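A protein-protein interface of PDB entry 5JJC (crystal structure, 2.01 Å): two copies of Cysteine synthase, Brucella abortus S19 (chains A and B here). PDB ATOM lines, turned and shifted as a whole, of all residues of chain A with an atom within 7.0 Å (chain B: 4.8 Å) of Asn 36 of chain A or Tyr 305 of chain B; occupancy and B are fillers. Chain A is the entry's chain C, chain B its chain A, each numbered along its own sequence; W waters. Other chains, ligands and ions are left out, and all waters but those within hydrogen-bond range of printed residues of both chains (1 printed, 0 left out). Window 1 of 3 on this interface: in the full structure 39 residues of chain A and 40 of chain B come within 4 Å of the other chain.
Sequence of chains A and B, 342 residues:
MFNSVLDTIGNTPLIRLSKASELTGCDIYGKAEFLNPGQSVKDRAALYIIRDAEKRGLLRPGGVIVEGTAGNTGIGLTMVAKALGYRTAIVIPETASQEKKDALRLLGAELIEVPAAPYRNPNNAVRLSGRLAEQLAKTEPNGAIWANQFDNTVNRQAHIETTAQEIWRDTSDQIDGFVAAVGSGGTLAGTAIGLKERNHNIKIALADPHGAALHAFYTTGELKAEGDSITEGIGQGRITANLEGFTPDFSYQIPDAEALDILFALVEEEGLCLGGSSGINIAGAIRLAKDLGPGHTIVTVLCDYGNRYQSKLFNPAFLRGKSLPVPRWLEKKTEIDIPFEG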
ATOM      1  N   THR A   8      -0.509  23.430  -4.120  1.00  0.00           N
ATOM      2  CA  THR A   8      -0.920  22.025  -3.986  1.00  0.00           C
ATOM      3  C   THR A   8      -0.147  21.320  -2.862  1.00  0.00           C
ATOM      4  O   THR A   8      -0.405  20.165  -2.557  1.00  0.00           O
ATOM      5  CB  THR A   8      -0.745  21.243  -5.306  1.00  0.00           C
ATOM      6  OG1 THR A   8       0.650  21.044  -5.586  1.00  0.00           O
ATOM      7  CG2 THR A   8      -1.422  22.002  -6.483  1.00  0.00           C
ATOM      8  N   ILE A   9       0.794  22.022  -2.243  1.00  0.00           N
ATOM      9  CA  ILE A   9       1.447  21.498  -1.034  1.00  0.00           C
ATOM     10  C   ILE A   9       0.447  21.471   0.127  1.00  0.00           C
ATOM     11  O   ILE A   9      -0.282  22.430   0.332  1.00  0.00           O
ATOM     12  CB  ILE A   9       2.667  22.350  -0.647  1.00  0.00           C
ATOM     13  CG1 ILE A   9       3.737  22.259  -1.742  1.00  0.00           C
ATOM     14  CG2 ILE A   9       3.224  21.929   0.717  1.00  0.00           C
ATOM     15  CD1 ILE A   9       4.920  23.167  -1.499  1.00  0.00           C
ATOM     16  N   GLY A  10       0.392  20.378   0.878  1.00  0.00           N
ATOM     17  CA  GLY A  10      -0.444  20.361   2.071  1.00  0.00           C
ATOM     18  C   GLY A  10      -1.879  19.936   1.804  1.00  0.00           C
ATOM     19  O   GLY A  10      -2.226  19.585   0.675  1.00  0.00           O
ATOM     20  N   ASN A  11      -2.716  19.974   2.839  1.00  0.00           N
ATOM     21  CA  ASN A  11      -4.091  19.465   2.745  1.00  0.00           C
ATOM     22  C   ASN A  11      -4.148  18.048   2.174  1.00  0.00           C
ATOM     23  O   ASN A  11      -5.001  17.725   1.341  1.00  0.00           O
ATOM     24  CB  ASN A  11      -4.952  20.417   1.909  1.00  0.00           C
ATOM     25  CG  ASN A  11      -5.233  21.726   2.641  1.00  0.00           C
ATOM     26  OD1 ASN A  11      -5.771  21.724   3.746  1.00  0.00           O
ATOM     27  ND2 ASN A  11      -4.836  22.838   2.044  1.00  0.00           N
ATOM     28  N   THR A  12      -3.218  17.211   2.625  1.00  0.00           N
ATOM     29  CA  THR A  12      -3.133  15.824   2.179  1.00  0.00           C
ATOM     30  C   THR A  12      -4.183  14.985   2.902  1.00  0.00           C
ATOM     31  O   THR A  12      -4.540  15.275   4.043  1.00  0.00           O
ATOM     32  CB  THR A  12      -1.740  15.247   2.439  1.00  0.00           C
ATOM     33  OG1 THR A  12      -1.421  15.425   3.824  1.00  0.00           O
ATOM     34  CG2 THR A  12      -0.694  15.976   1.583  1.00  0.00           C
ATOM     35  N   ALA A  32      -1.302  11.174   3.893  1.00  0.00           N
ATOM     36  CA  ALA A  32      -0.678  10.861   2.607  1.00  0.00           C
ATOM     37  C   ALA A  32       0.241  11.964   2.088  1.00  0.00           C
ATOM     38  O   ALA A  32      -0.061  12.618   1.082  1.00  0.00           O
ATOM     39  CB  ALA A  32      -1.765  10.554   1.563  1.00  0.00           C
ATOM     40  N   GLU A  33       1.380  12.132   2.757  1.00  0.00           N
ATOM     41  CA  GLU A  33       2.350  13.162   2.417  1.00  0.00           C
ATOM     42  C   GLU A  33       3.043  12.889   1.099  1.00  0.00           C
ATOM     43  O   GLU A  33       3.686  13.784   0.548  1.00  0.00           O
ATOM     44  CB  GLU A  33       3.403  13.299   3.530  1.00  0.00           C
ATOM     45  CG  GLU A  33       2.847  13.928   4.794  1.00  0.00           C
ATOM     46  CD  GLU A  33       2.231  15.288   4.538  1.00  0.00           C
ATOM     47  OE1 GLU A  33       2.973  16.206   4.135  1.00  0.00           O
ATOM     48  OE2 GLU A  33       1.011  15.452   4.757  1.00  0.00           O
ATOM     49  N   PHE A  34       2.923  11.655   0.599  1.00  0.00           N
ATOM     50  CA  PHE A  34       3.438  11.324  -0.730  1.00  0.00           C
ATOM     51  C   PHE A  34       2.626  12.015  -1.842  1.00  0.00           C
ATOM     52  O   PHE A  34       3.093  12.142  -2.978  1.00  0.00           O
ATOM     53  CB  PHE A  34       3.469   9.796  -0.941  1.00  0.00           C
ATOM     54  CG  PHE A  34       2.131   9.098  -0.750  1.00  0.00           C
ATOM     55  CD1 PHE A  34       1.240   8.957  -1.807  1.00  0.00           C
ATOM     56  CD2 PHE A  34       1.804   8.512   0.468  1.00  0.00           C
ATOM     57  CE1 PHE A  34       0.026   8.281  -1.645  1.00  0.00           C
ATOM     58  CE2 PHE A  34       0.590   7.846   0.645  1.00  0.00           C
ATOM     59  CZ  PHE A  34      -0.301   7.726  -0.419  1.00  0.00           C
ATOM     60  N   LEU A  35       1.432  12.502  -1.506  1.00  0.00           N
ATOM     61  CA  LEU A  35       0.612  13.227  -2.473  1.00  0.00           C
ATOM     62  C   LEU A  35       0.917  14.750  -2.528  1.00  0.00           C
ATOM     63  O   LEU A  35       0.160  15.517  -3.122  1.00  0.00           O
ATOM     64  CB  LEU A  35      -0.874  13.011  -2.171  1.00  0.00           C
ATOM     65  CG  LEU A  35      -1.428  11.597  -2.361  1.00  0.00           C
ATOM     66  CD1 LEU A  35      -2.927  11.532  -2.039  1.00  0.00           C
ATOM     67  CD2 LEU A  35      -1.176  11.112  -3.788  1.00  0.00           C
ATOM     68  N   ASN A  36       2.008  15.183  -1.906  1.00  0.00           N
ATOM     69  CA  ASN A  36       2.533  16.530  -2.152  1.00  0.00           C
ATOM     70  C   ASN A  36       3.212  16.558  -3.520  1.00  0.00           C
ATOM     71  O   ASN A  36       3.627  15.514  -4.028  1.00  0.00           O
ATOM     72  CB  ASN A  36       3.510  16.952  -1.052  1.00  0.00           C
ATOM     73  CG  ASN A  36       2.812  17.293   0.247  1.00  0.00           C
ATOM     74  OD1 ASN A  36       1.820  18.025   0.269  1.00  0.00           O
ATOM     75  ND2 ASN A  36       3.325  16.757   1.341  1.00  0.00           N
ATOM     76  N   PRO A  37       3.325  17.739  -4.134  1.00  0.00           N
ATOM     77  CA  PRO A  37       3.881  17.748  -5.494  1.00  0.00           C
ATOM     78  C   PRO A  37       5.378  17.400  -5.561  1.00  0.00           C
ATOM     79  O   PRO A  37       5.846  16.984  -6.619  1.00  0.00           O
ATOM     80  CB  PRO A  37       3.631  19.180  -5.962  1.00  0.00           C
ATOM     81  CG  PRO A  37       3.586  19.988  -4.678  1.00  0.00           C
ATOM     82  CD  PRO A  37       2.909  19.086  -3.688  1.00  0.00           C
ATOM     83  N   GLY A  38       6.106  17.560  -4.459  1.00  0.00           N
ATOM     84  CA  GLY A  38       7.491  17.106  -4.387  1.00  0.00           C
ATOM     85  C   GLY A  38       7.560  15.649  -3.958  1.00  0.00           C
ATOM     86  O   GLY A  38       8.644  15.075  -3.800  1.00  0.00           O
ATOM     87  N   GLN A  39       6.381  15.061  -3.756  1.00  0.00           N
ATOM     88  CA  GLN A  39       6.207  13.635  -3.444  1.00  0.00           C
ATOM     89  C   GLN A  39       6.720  13.197  -2.078  1.00  0.00           C
ATOM     90  O   GLN A  39       6.942  12.009  -1.856  1.00  0.00           O
ATOM     91  CB  GLN A  39       6.867  12.770  -4.516  1.00  0.00           C
ATOM     92  CG  GLN A  39       6.549  13.216  -5.924  1.00  0.00           C
ATOM     93  CD  GLN A  39       6.566  12.063  -6.879  1.00  0.00           C
ATOM     94  OE1 GLN A  39       7.576  11.779  -7.507  1.00  0.00           O
ATOM     95  NE2 GLN A  39       5.440  11.376  -6.983  1.00  0.00           N
ATOM     96  N   SER A  40       6.896  14.141  -1.158  1.00  0.00           N
ATOM     97  CA  SER A  40       7.211  13.772   0.227  1.00  0.00           C
ATOM     98  C   SER A  40       6.736  14.824   1.207  1.00  0.00           C
ATOM     99  O   SER A  40       6.350  15.934   0.820  1.00  0.00           O
ATOM    100  CB  SER A  40       8.720  13.558   0.426  1.00  0.00           C
ATOM    101  OG  SER A  40       9.370  14.803   0.639  1.00  0.00           O
ATOM    102  N   VAL A  41       6.795  14.455   2.480  1.00  0.00           N
ATOM    103  CA  VAL A  41       6.503  15.336   3.601  1.00  0.00           C
ATOM    104  C   VAL A  41       7.361  16.616   3.589  1.00  0.00           C
ATOM    105  O   VAL A  41       6.947  17.649   4.127  1.00  0.00           O
ATOM    106  CB  VAL A  41       6.710  14.571   4.941  1.00  0.00           C
ATOM    107  CG1 VAL A  41       8.184  14.173   5.128  1.00  0.00           C
ATOM    108  CG2 VAL A  41       6.187  15.370   6.144  1.00  0.00           C
ATOM    109  N1  LLP A  42      10.374  10.228   6.311  1.00  0.00           N
ATOM    110  C2  LLP A  42      10.887  10.743   5.203  1.00  0.00           C
ATOM    111  C2' LLP A  42      10.792   9.933   3.884  1.00  0.00           C
ATOM    112  C3  LLP A  42      11.523  12.023   5.237  1.00  0.00           C
ATOM    113  O3  LLP A  42      12.056  12.529   4.051  1.00  0.00           O
ATOM    114  C4  LLP A  42      11.604  12.729   6.425  1.00  0.00           C
ATOM    115  C4' LLP A  42      12.312  14.173   6.506  1.00  0.00           C
ATOM    116  C5  LLP A  42      11.070  12.182   7.563  1.00  0.00           C
ATOM    117  C6  LLP A  42      10.455  10.929   7.509  1.00  0.00           C
ATOM    118  C5' LLP A  42      11.127  12.875   8.957  1.00  0.00           C
ATOM    119  OP4 LLP A  42      10.548  14.151   8.952  1.00  0.00           O
ATOM    120  P   LLP A  42      11.144  15.241   9.881  1.00  0.00           P
ATOM    121  OP1 LLP A  42      12.444  15.743   9.254  1.00  0.00           O
ATOM    122  OP2 LLP A  42      10.125  16.326   9.974  1.00  0.00           O
ATOM    123  OP3 LLP A  42      11.467  14.677  11.221  1.00  0.00           O
ATOM    124  N   LLP A  42       8.534  16.553   2.956  1.00  0.00           N
ATOM    125  CA  LLP A  42       9.524  17.657   3.018  1.00  0.00           C
ATOM    126  CB  LLP A  42      10.857  17.243   2.419  1.00  0.00           C
ATOM    127  CG  LLP A  42      11.644  16.254   3.285  1.00  0.00           C
ATOM    128  CD  LLP A  42      11.821  16.776   4.723  1.00  0.00           C
ATOM    129  CE  LLP A  42      13.035  16.071   5.373  1.00  0.00           C
ATOM    130  NZ  LLP A  42      12.897  14.611   5.284  1.00  0.00           N
ATOM    131  C   LLP A  42       9.059  18.884   2.302  1.00  0.00           C
ATOM    132  O   LLP A  42       9.643  19.941   2.500  1.00  0.00           O
ATOM    133  N   ASP A  43       8.019  18.772   1.469  1.00  0.00           N
ATOM    134  CA  ASP A  43       7.449  19.947   0.801  1.00  0.00           C
ATOM    135  C   ASP A  43       7.031  21.026   1.787  1.00  0.00           C
ATOM    136  O   ASP A  43       7.112  22.226   1.491  1.00  0.00           O
ATOM    137  CB  ASP A  43       6.232  19.558  -0.041  1.00  0.00           C
ATOM    138  CG  ASP A  43       6.613  18.948  -1.377  1.00  0.00           C
ATOM    139  OD1 ASP A  43       7.790  18.552  -1.546  1.00  0.00           O
ATOM    140  OD2 ASP A  43       5.722  18.859  -2.255  1.00  0.00           O
ATOM    141  N   ARG A  44       6.579  20.604   2.962  1.00  0.00           N
ATOM    142  CA  ARG A  44       6.091  21.548   3.963  1.00  0.00           C
ATOM    143  C   ARG A  44       7.211  22.400   4.571  1.00  0.00           C
ATOM    144  O   ARG A  44       7.114  23.626   4.584  1.00  0.00           O
ATOM    145  CB  ARG A  44       5.340  20.804   5.063  1.00  0.00           C
ATOM    146  CG  ARG A  44       3.993  20.190   4.603  1.00  0.00           C
ATOM    147  CD  ARG A  44       3.369  19.359   5.739  1.00  0.00           C
ATOM    148  NE  ARG A  44       2.246  18.542   5.287  1.00  0.00           N
ATOM    149  CZ  ARG A  44       0.981  18.947   5.237  1.00  0.00           C
ATOM    150  NH1 ARG A  44       0.643  20.177   5.617  1.00  0.00           N
ATOM    151  NH2 ARG A  44       0.044  18.114   4.800  1.00  0.00           N
ATOM    152  N   MET A  79      12.252  22.051  -5.898  1.00  0.00           N
ATOM    153  CA  MET A  79      10.948  22.326  -6.493  1.00  0.00           C
ATOM    154  C   MET A  79      10.393  23.691  -6.066  1.00  0.00           C
ATOM    155  O   MET A  79       9.929  24.468  -6.902  1.00  0.00           O
ATOM    156  CB  MET A  79       9.931  21.247  -6.134  1.00  0.00           C
ATOM    157  CG  MET A  79       8.523  21.665  -6.509  1.00  0.00           C
ATOM    158  SD  MET A  79       7.255  20.574  -5.869  1.00  0.00           S
ATOM    159  CE  MET A  79       7.232  21.087  -4.144  1.00  0.00           C
ATOM    160  N   LEU A 106      17.774  16.370 -12.024  1.00  0.00           N
ATOM    161  CA  LEU A 106      16.576  16.368 -12.865  1.00  0.00           C
ATOM    162  C   LEU A 106      15.757  17.649 -12.692  1.00  0.00           C
ATOM    163  O   LEU A 106      15.326  18.271 -13.665  1.00  0.00           O
ATOM    164  CB  LEU A 106      15.697  15.157 -12.533  1.00  0.00           C
ATOM    165  CG  LEU A 106      14.360  15.130 -13.285  1.00  0.00           C
ATOM    166  CD1 LEU A 106      14.612  14.789 -14.739  1.00  0.00           C
ATOM    167  CD2 LEU A 106      13.347  14.168 -12.673  1.00  0.00           C
ATOM    168  N   CYS A 303       5.173   9.093   4.589  1.00  0.00           N
ATOM    169  CA  CYS A 303       6.037  10.230   4.285  1.00  0.00           C
ATOM    170  C   CYS A 303       6.382  10.397   2.822  1.00  0.00           C
ATOM    171  O   CYS A 303       6.535  11.527   2.365  1.00  0.00           O
ATOM    172  CB  CYS A 303       7.335  10.127   5.095  1.00  0.00           C
ATOM    173  SG  CYS A 303       7.034   9.833   6.853  1.00  0.00           S
ATOM    174  N   TYR A 305       6.840   7.877  -1.282  1.00  0.00           N
ATOM    175  CA  TYR A 305       6.675   6.651  -2.067  1.00  0.00           C
ATOM    176  C   TYR A 305       7.878   5.734  -1.956  1.00  0.00           C
ATOM    177  O   TYR A 305       8.972   6.185  -1.656  1.00  0.00           O
ATOM    178  CB  TYR A 305       6.483   6.967  -3.543  1.00  0.00           C
ATOM    179  CG  TYR A 305       5.139   7.506  -3.947  1.00  0.00           C
ATOM    180  CD1 TYR A 305       4.019   6.696  -3.950  1.00  0.00           C
ATOM    181  CD2 TYR A 305       5.004   8.823  -4.387  1.00  0.00           C
ATOM    182  CE1 TYR A 305       2.785   7.180  -4.358  1.00  0.00           C
ATOM    183  CE2 TYR A 305       3.768   9.324  -4.793  1.00  0.00           C
ATOM    184  CZ  TYR A 305       2.671   8.491  -4.779  1.00  0.00           C
ATOM    185  OH  TYR A 305       1.458   8.966  -5.188  1.00  0.00           O
ATOM    186  N   PHE B  34      -0.897  14.049 -12.133  1.00  0.00           N
ATOM    187  CA  PHE B  34       0.247  13.409 -11.484  1.00  0.00           C
ATOM    188  C   PHE B  34       0.022  13.279  -9.971  1.00  0.00           C
ATOM    189  O   PHE B  34       0.664  12.451  -9.320  1.00  0.00           O
ATOM    190  CB  PHE B  34       1.569  14.158 -11.781  1.00  0.00           C
ATOM    191  CG  PHE B  34       1.556  15.633 -11.437  1.00  0.00           C
ATOM    192  CD1 PHE B  34       1.904  16.066 -10.166  1.00  0.00           C
ATOM    193  CD2 PHE B  34       1.250  16.585 -12.402  1.00  0.00           C
ATOM    194  CE1 PHE B  34       1.924  17.415  -9.848  1.00  0.00           C
ATOM    195  CE2 PHE B  34       1.269  17.943 -12.090  1.00  0.00           C
ATOM    196  CZ  PHE B  34       1.596  18.356 -10.809  1.00  0.00           C
ATOM    197  N   LEU B  35      -0.905  14.057  -9.412  1.00  0.00           N
ATOM    198  CA  LEU B  35      -1.176  13.958  -7.973  1.00  0.00           C
ATOM    199  C   LEU B  35      -2.186  12.860  -7.588  1.00  0.00           C
ATOM    200  O   LEU B  35      -2.639  12.807  -6.447  1.00  0.00           O
ATOM    201  CB  LEU B  35      -1.656  15.301  -7.424  1.00  0.00           C
ATOM    202  CG  LEU B  35      -0.580  16.393  -7.510  1.00  0.00           C
ATOM    203  CD1 LEU B  35      -1.153  17.730  -7.068  1.00  0.00           C
ATOM    204  CD2 LEU B  35       0.653  16.000  -6.675  1.00  0.00           C
ATOM    205  N   GLN B  39       0.125   8.062  -9.492  1.00  0.00           N
ATOM    206  CA  GLN B  39       1.007   9.074 -10.094  1.00  0.00           C
ATOM    207  C   GLN B  39       0.749   9.329 -11.595  1.00  0.00           C
ATOM    208  O   GLN B  39       1.612   9.861 -12.300  1.00  0.00           O
ATOM    209  CB  GLN B  39       2.484   8.700  -9.865  1.00  0.00           C
ATOM    210  CG  GLN B  39       2.837   8.447  -8.368  1.00  0.00           C
ATOM    211  CD  GLN B  39       4.304   8.051  -8.135  1.00  0.00           C
ATOM    212  OE1 GLN B  39       5.217   8.758  -8.529  1.00  0.00           O
ATOM    213  NE2 GLN B  39       4.515   6.915  -7.489  1.00  0.00           N
ATOM    214  N   CYS B 273       8.020  19.273 -13.126  1.00  0.00           N
ATOM    215  CA  CYS B 273       8.789  18.349 -13.952  1.00  0.00           C
ATOM    216  C   CYS B 273       7.867  17.231 -14.408  1.00  0.00           C
ATOM    217  O   CYS B 273       7.532  16.332 -13.626  1.00  0.00           O
ATOM    218  CB  CYS B 273       9.981  17.775 -13.191  1.00  0.00           C
ATOM    219  SG  CYS B 273      10.998  16.684 -14.220  1.00  0.00           S
ATOM    220  N   LEU B 274       7.439  17.304 -15.664  1.00  0.00           N
ATOM    221  CA  LEU B 274       6.347  16.472 -16.146  1.00  0.00           C
ATOM    222  C   LEU B 274       6.746  15.554 -17.301  1.00  0.00           C
ATOM    223  O   LEU B 274       7.831  15.686 -17.876  1.00  0.00           O
ATOM    224  CB  LEU B 274       5.180  17.364 -16.588  1.00  0.00           C
ATOM    225  CG  LEU B 274       4.718  18.419 -15.580  1.00  0.00           C
ATOM    226  CD1 LEU B 274       3.698  19.358 -16.212  1.00  0.00           C
ATOM    227  CD2 LEU B 274       4.140  17.743 -14.321  1.00  0.00           C
ATOM    228  N   GLY B 275       5.846  14.633 -17.646  1.00  0.00           N
ATOM    229  CA  GLY B 275       6.114  13.653 -18.682  1.00  0.00           C
ATOM    230  C   GLY B 275       5.942  14.246 -20.065  1.00  0.00           C
ATOM    231  O   GLY B 275       5.460  15.365 -20.209  1.00  0.00           O
ATOM    232  N   ASP B 304       1.464  13.003 -15.966  1.00  0.00           N
ATOM    233  CA  ASP B 304       2.325  12.287 -15.021  1.00  0.00           C
ATOM    234  C   ASP B 304       3.641  13.038 -14.820  1.00  0.00           C
ATOM    235  O   ASP B 304       3.845  14.092 -15.413  1.00  0.00           O
ATOM    236  CB  ASP B 304       2.573  10.818 -15.477  1.00  0.00           C
ATOM    237  CG  ASP B 304       3.306  10.696 -16.826  1.00  0.00           C
ATOM    238  OD1 ASP B 304       3.673  11.707 -17.460  1.00  0.00           O
ATOM    239  OD2 ASP B 304       3.541   9.542 -17.251  1.00  0.00           O
ATOM    240  N   TYR B 305       4.516  12.504 -13.967  1.00  0.00           N
ATOM    241  CA  TYR B 305       5.805  13.136 -13.637  1.00  0.00           C
ATOM    242  C   TYR B 305       6.915  12.861 -14.658  1.00  0.00           C
ATOM    243  O   TYR B 305       6.978  11.782 -15.232  1.00  0.00           O
ATOM    244  CB  TYR B 305       6.308  12.645 -12.275  1.00  0.00           C
ATOM    245  CG  TYR B 305       5.649  13.247 -11.061  1.00  0.00           C
ATOM    246  CD1 TYR B 305       6.041  14.492 -10.573  1.00  0.00           C
ATOM    247  CD2 TYR B 305       4.669  12.550 -10.365  1.00  0.00           C
ATOM    248  CE1 TYR B 305       5.453  15.034  -9.442  1.00  0.00           C
ATOM    249  CE2 TYR B 305       4.077  13.080  -9.231  1.00  0.00           C
ATOM    250  CZ  TYR B 305       4.473  14.325  -8.774  1.00  0.00           C
ATOM    251  OH  TYR B 305       3.886  14.857  -7.653  1.00  0.00           O
ATOM    252  N   GLY B 306       7.832  13.809 -14.821  1.00  0.00           N
ATOM    253  CA  GLY B 306       9.015  13.586 -15.639  1.00  0.00           C
ATOM    254  C   GLY B 306       9.957  12.488 -15.155  1.00  0.00           C
ATOM    255  O   GLY B 306      10.691  11.893 -15.959  1.00  0.00           O
ATOM    256  N   ASN B 307       9.952  12.204 -13.852  1.00  0.00           N
ATOM    257  CA  ASN B 307      10.897  11.225 -13.304  1.00  0.00           C
ATOM    258  C   ASN B 307      10.560   9.827 -13.796  1.00  0.00           C
ATOM    259  O   ASN B 307      11.380   8.913 -13.763  1.00  0.00           O
ATOM    260  CB  ASN B 307      10.935  11.276 -11.763  1.00  0.00           C
ATOM    261  CG  ASN B 307       9.589  10.968 -11.114  1.00  0.00           C
ATOM    262  OD1 ASN B 307       8.916   9.993 -11.457  1.00  0.00           O
ATOM    263  ND2 ASN B 307       9.197  11.804 -10.160  1.00  0.00           N
ATOM    264  N   ARG B 308       9.346   9.680 -14.297  1.00  0.00           N
ATOM    265  CA  ARG B 308       8.935   8.434 -14.905  1.00  0.00           C
ATOM    266  C   ARG B 308       9.624   8.214 -16.271  1.00  0.00           C
ATOM    267  O   ARG B 308       9.403   7.202 -16.928  1.00  0.00           O
ATOM    268  CB  ARG B 308       7.394   8.442 -15.025  1.00  0.00           C
ATOM    269  CG  ARG B 308       6.720   7.148 -15.450  1.00  0.00           C
ATOM    270  CD  ARG B 308       5.309   7.003 -14.837  1.00  0.00           C
ATOM    271  NE  ARG B 308       5.423   6.560 -13.451  1.00  0.00           N
ATOM    272  CZ  ARG B 308       4.405   6.262 -12.648  1.00  0.00           C
ATOM    273  NH1 ARG B 308       3.138   6.354 -13.068  1.00  0.00           N
ATOM    274  NH2 ARG B 308       4.666   5.867 -11.409  1.00  0.00           N
ATOM    275  N   TYR B 309      10.470   9.148 -16.703  1.00  0.00           N
ATOM    276  CA  TYR B 309      11.026   9.111 -18.073  1.00  0.00           C
ATOM    277  C   TYR B 309      12.485   9.545 -18.146  1.00  0.00           C
ATOM    278  O   TYR B 309      12.936  10.053 -19.119  1.00  0.00           O
ATOM    279  CB  TYR B 309      10.267  10.040 -18.988  1.00  0.00           C
ATOM    280  CG  TYR B 309       8.816   9.784 -19.075  1.00  0.00           C
ATOM    281  CD1 TYR B 309       8.314   8.890 -20.002  1.00  0.00           C
ATOM    282  CD2 TYR B 309       7.940  10.419 -18.220  1.00  0.00           C
ATOM    283  CE1 TYR B 309       6.961   8.654 -20.088  1.00  0.00           C
ATOM    284  CE2 TYR B 309       6.584  10.197 -18.300  1.00  0.00           C
ATOM    285  CZ  TYR B 309       6.095   9.311 -19.241  1.00  0.00           C
ATOM    286  OH  TYR B 309       4.737   9.049 -19.357  1.00  0.00           O
HETATM  287  O   HOH W   1       1.421  11.166  -6.713  1.00  0.00           O
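The side-chain amide nitrogen (NE2) of Gln 39 of chain A is in hydrogen-bond range of the side-chain amide oxygen (OE1) of Gln 39 of chain B, 3.0 Å away.
The side-chain hydroxyl of Tyr 305 of chain B sits at hydrogen-bond distance from the backbone carbonyl oxygen of Pro 37 of chain A (3.1 Å).
The side-chain amide nitrogen (ND2) of Asn 307 of chain B sits at hydrogen-bond distance from the side-chain amide oxygen (OE1) of Gln 39 of chain A (3.1 Å).
Of the 12 printed residues of chain B, 5 touch a printed residue of chain A.
Printed residues of chain B that touch a printed residue of chain A: Leu 35, Gln 39, Cys 273, Tyr 305 and Asn 307.
Hydrophobic or aromatic side chains of chain B within 4 Å of the printed part of chain A: Leu 35 and Tyr 305.
Glu 33 of chain A touches none of the printed residues of chain B.
Of the printed residues of chain B, Leu 35 of chain A touches Leu 35 (3.5 Å).
Printed residues of chain B within 4 Å of Asn 36 of chain A: Tyr 305.
Of the printed residues of chain A, Leu 35 of chain B touches Thr 8 (3.95 Å), Leu 35 (3.5 Å) and Pro 37 (3.9 Å).
Of the printed residues of chain A, Tyr 305 of chain B touches Asn 36, Pro 37 and Gln 39.
Tyr 309 of chain B touches none of the printed residues of chain A.
The backbone NH of Gly 306 of chain B is in hydrogen-bond range of the backbone carbonyl oxygen of Cys 273 of chain B, 2.8 Å away.
N of Gly 10 of chain A lies within hydrogen-bond range of OD1 of Asn 36 of chain A (2.8 Å).
The side-chain carboxylate (OE1) of Glu 33 of chain A is in hydrogen-bond range of the side-chain amide nitrogen (ND2) of Asn 36 of chain A, 2.9 Å away.
ND2 of Asn 36 of chain A is in hydrogen-bond range of O of Ser 40 of chain A, at 3.2 Å.
Water W1 bridges OH of Tyr 305 of chain A and O of Phe 34 of chain B.
Among the printed residues, pairs that only touch across the chains: Gln 39 of chain A with Tyr 305 of chain B (3.1 Å), Leu 35 of chain A with Leu 35 of chain B (3.5 Å), Tyr 305 of chain A with Gln 39 of chain B (3.5 Å), Asn 36 of chain A with Tyr 305 of chain B (3.7 Å), Leu 106 of chain A with Cys 273 of chain B (3.8 Å), Pro 37 of chain A with Leu 35 of chain B (3.9 Å), Leu 106 of chain A with Asn 307 of chain B (3.9 Å) and Thr 8 of chain A with Leu 35 of chain B (3.95 Å).
Leu 35 of chain B touches its own counterpart, Leu 35 of chain A.
Gln 39 of chain B touches its own counterpart, Gln 39 of chain A.
Gln 39 of chain A touches Tyr 305 of chain B, and with the chains exchanged Tyr 305 of chain A touches Gln 39 of chain B.
Positions printed for both chains: 34, 35, 39 and 305.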
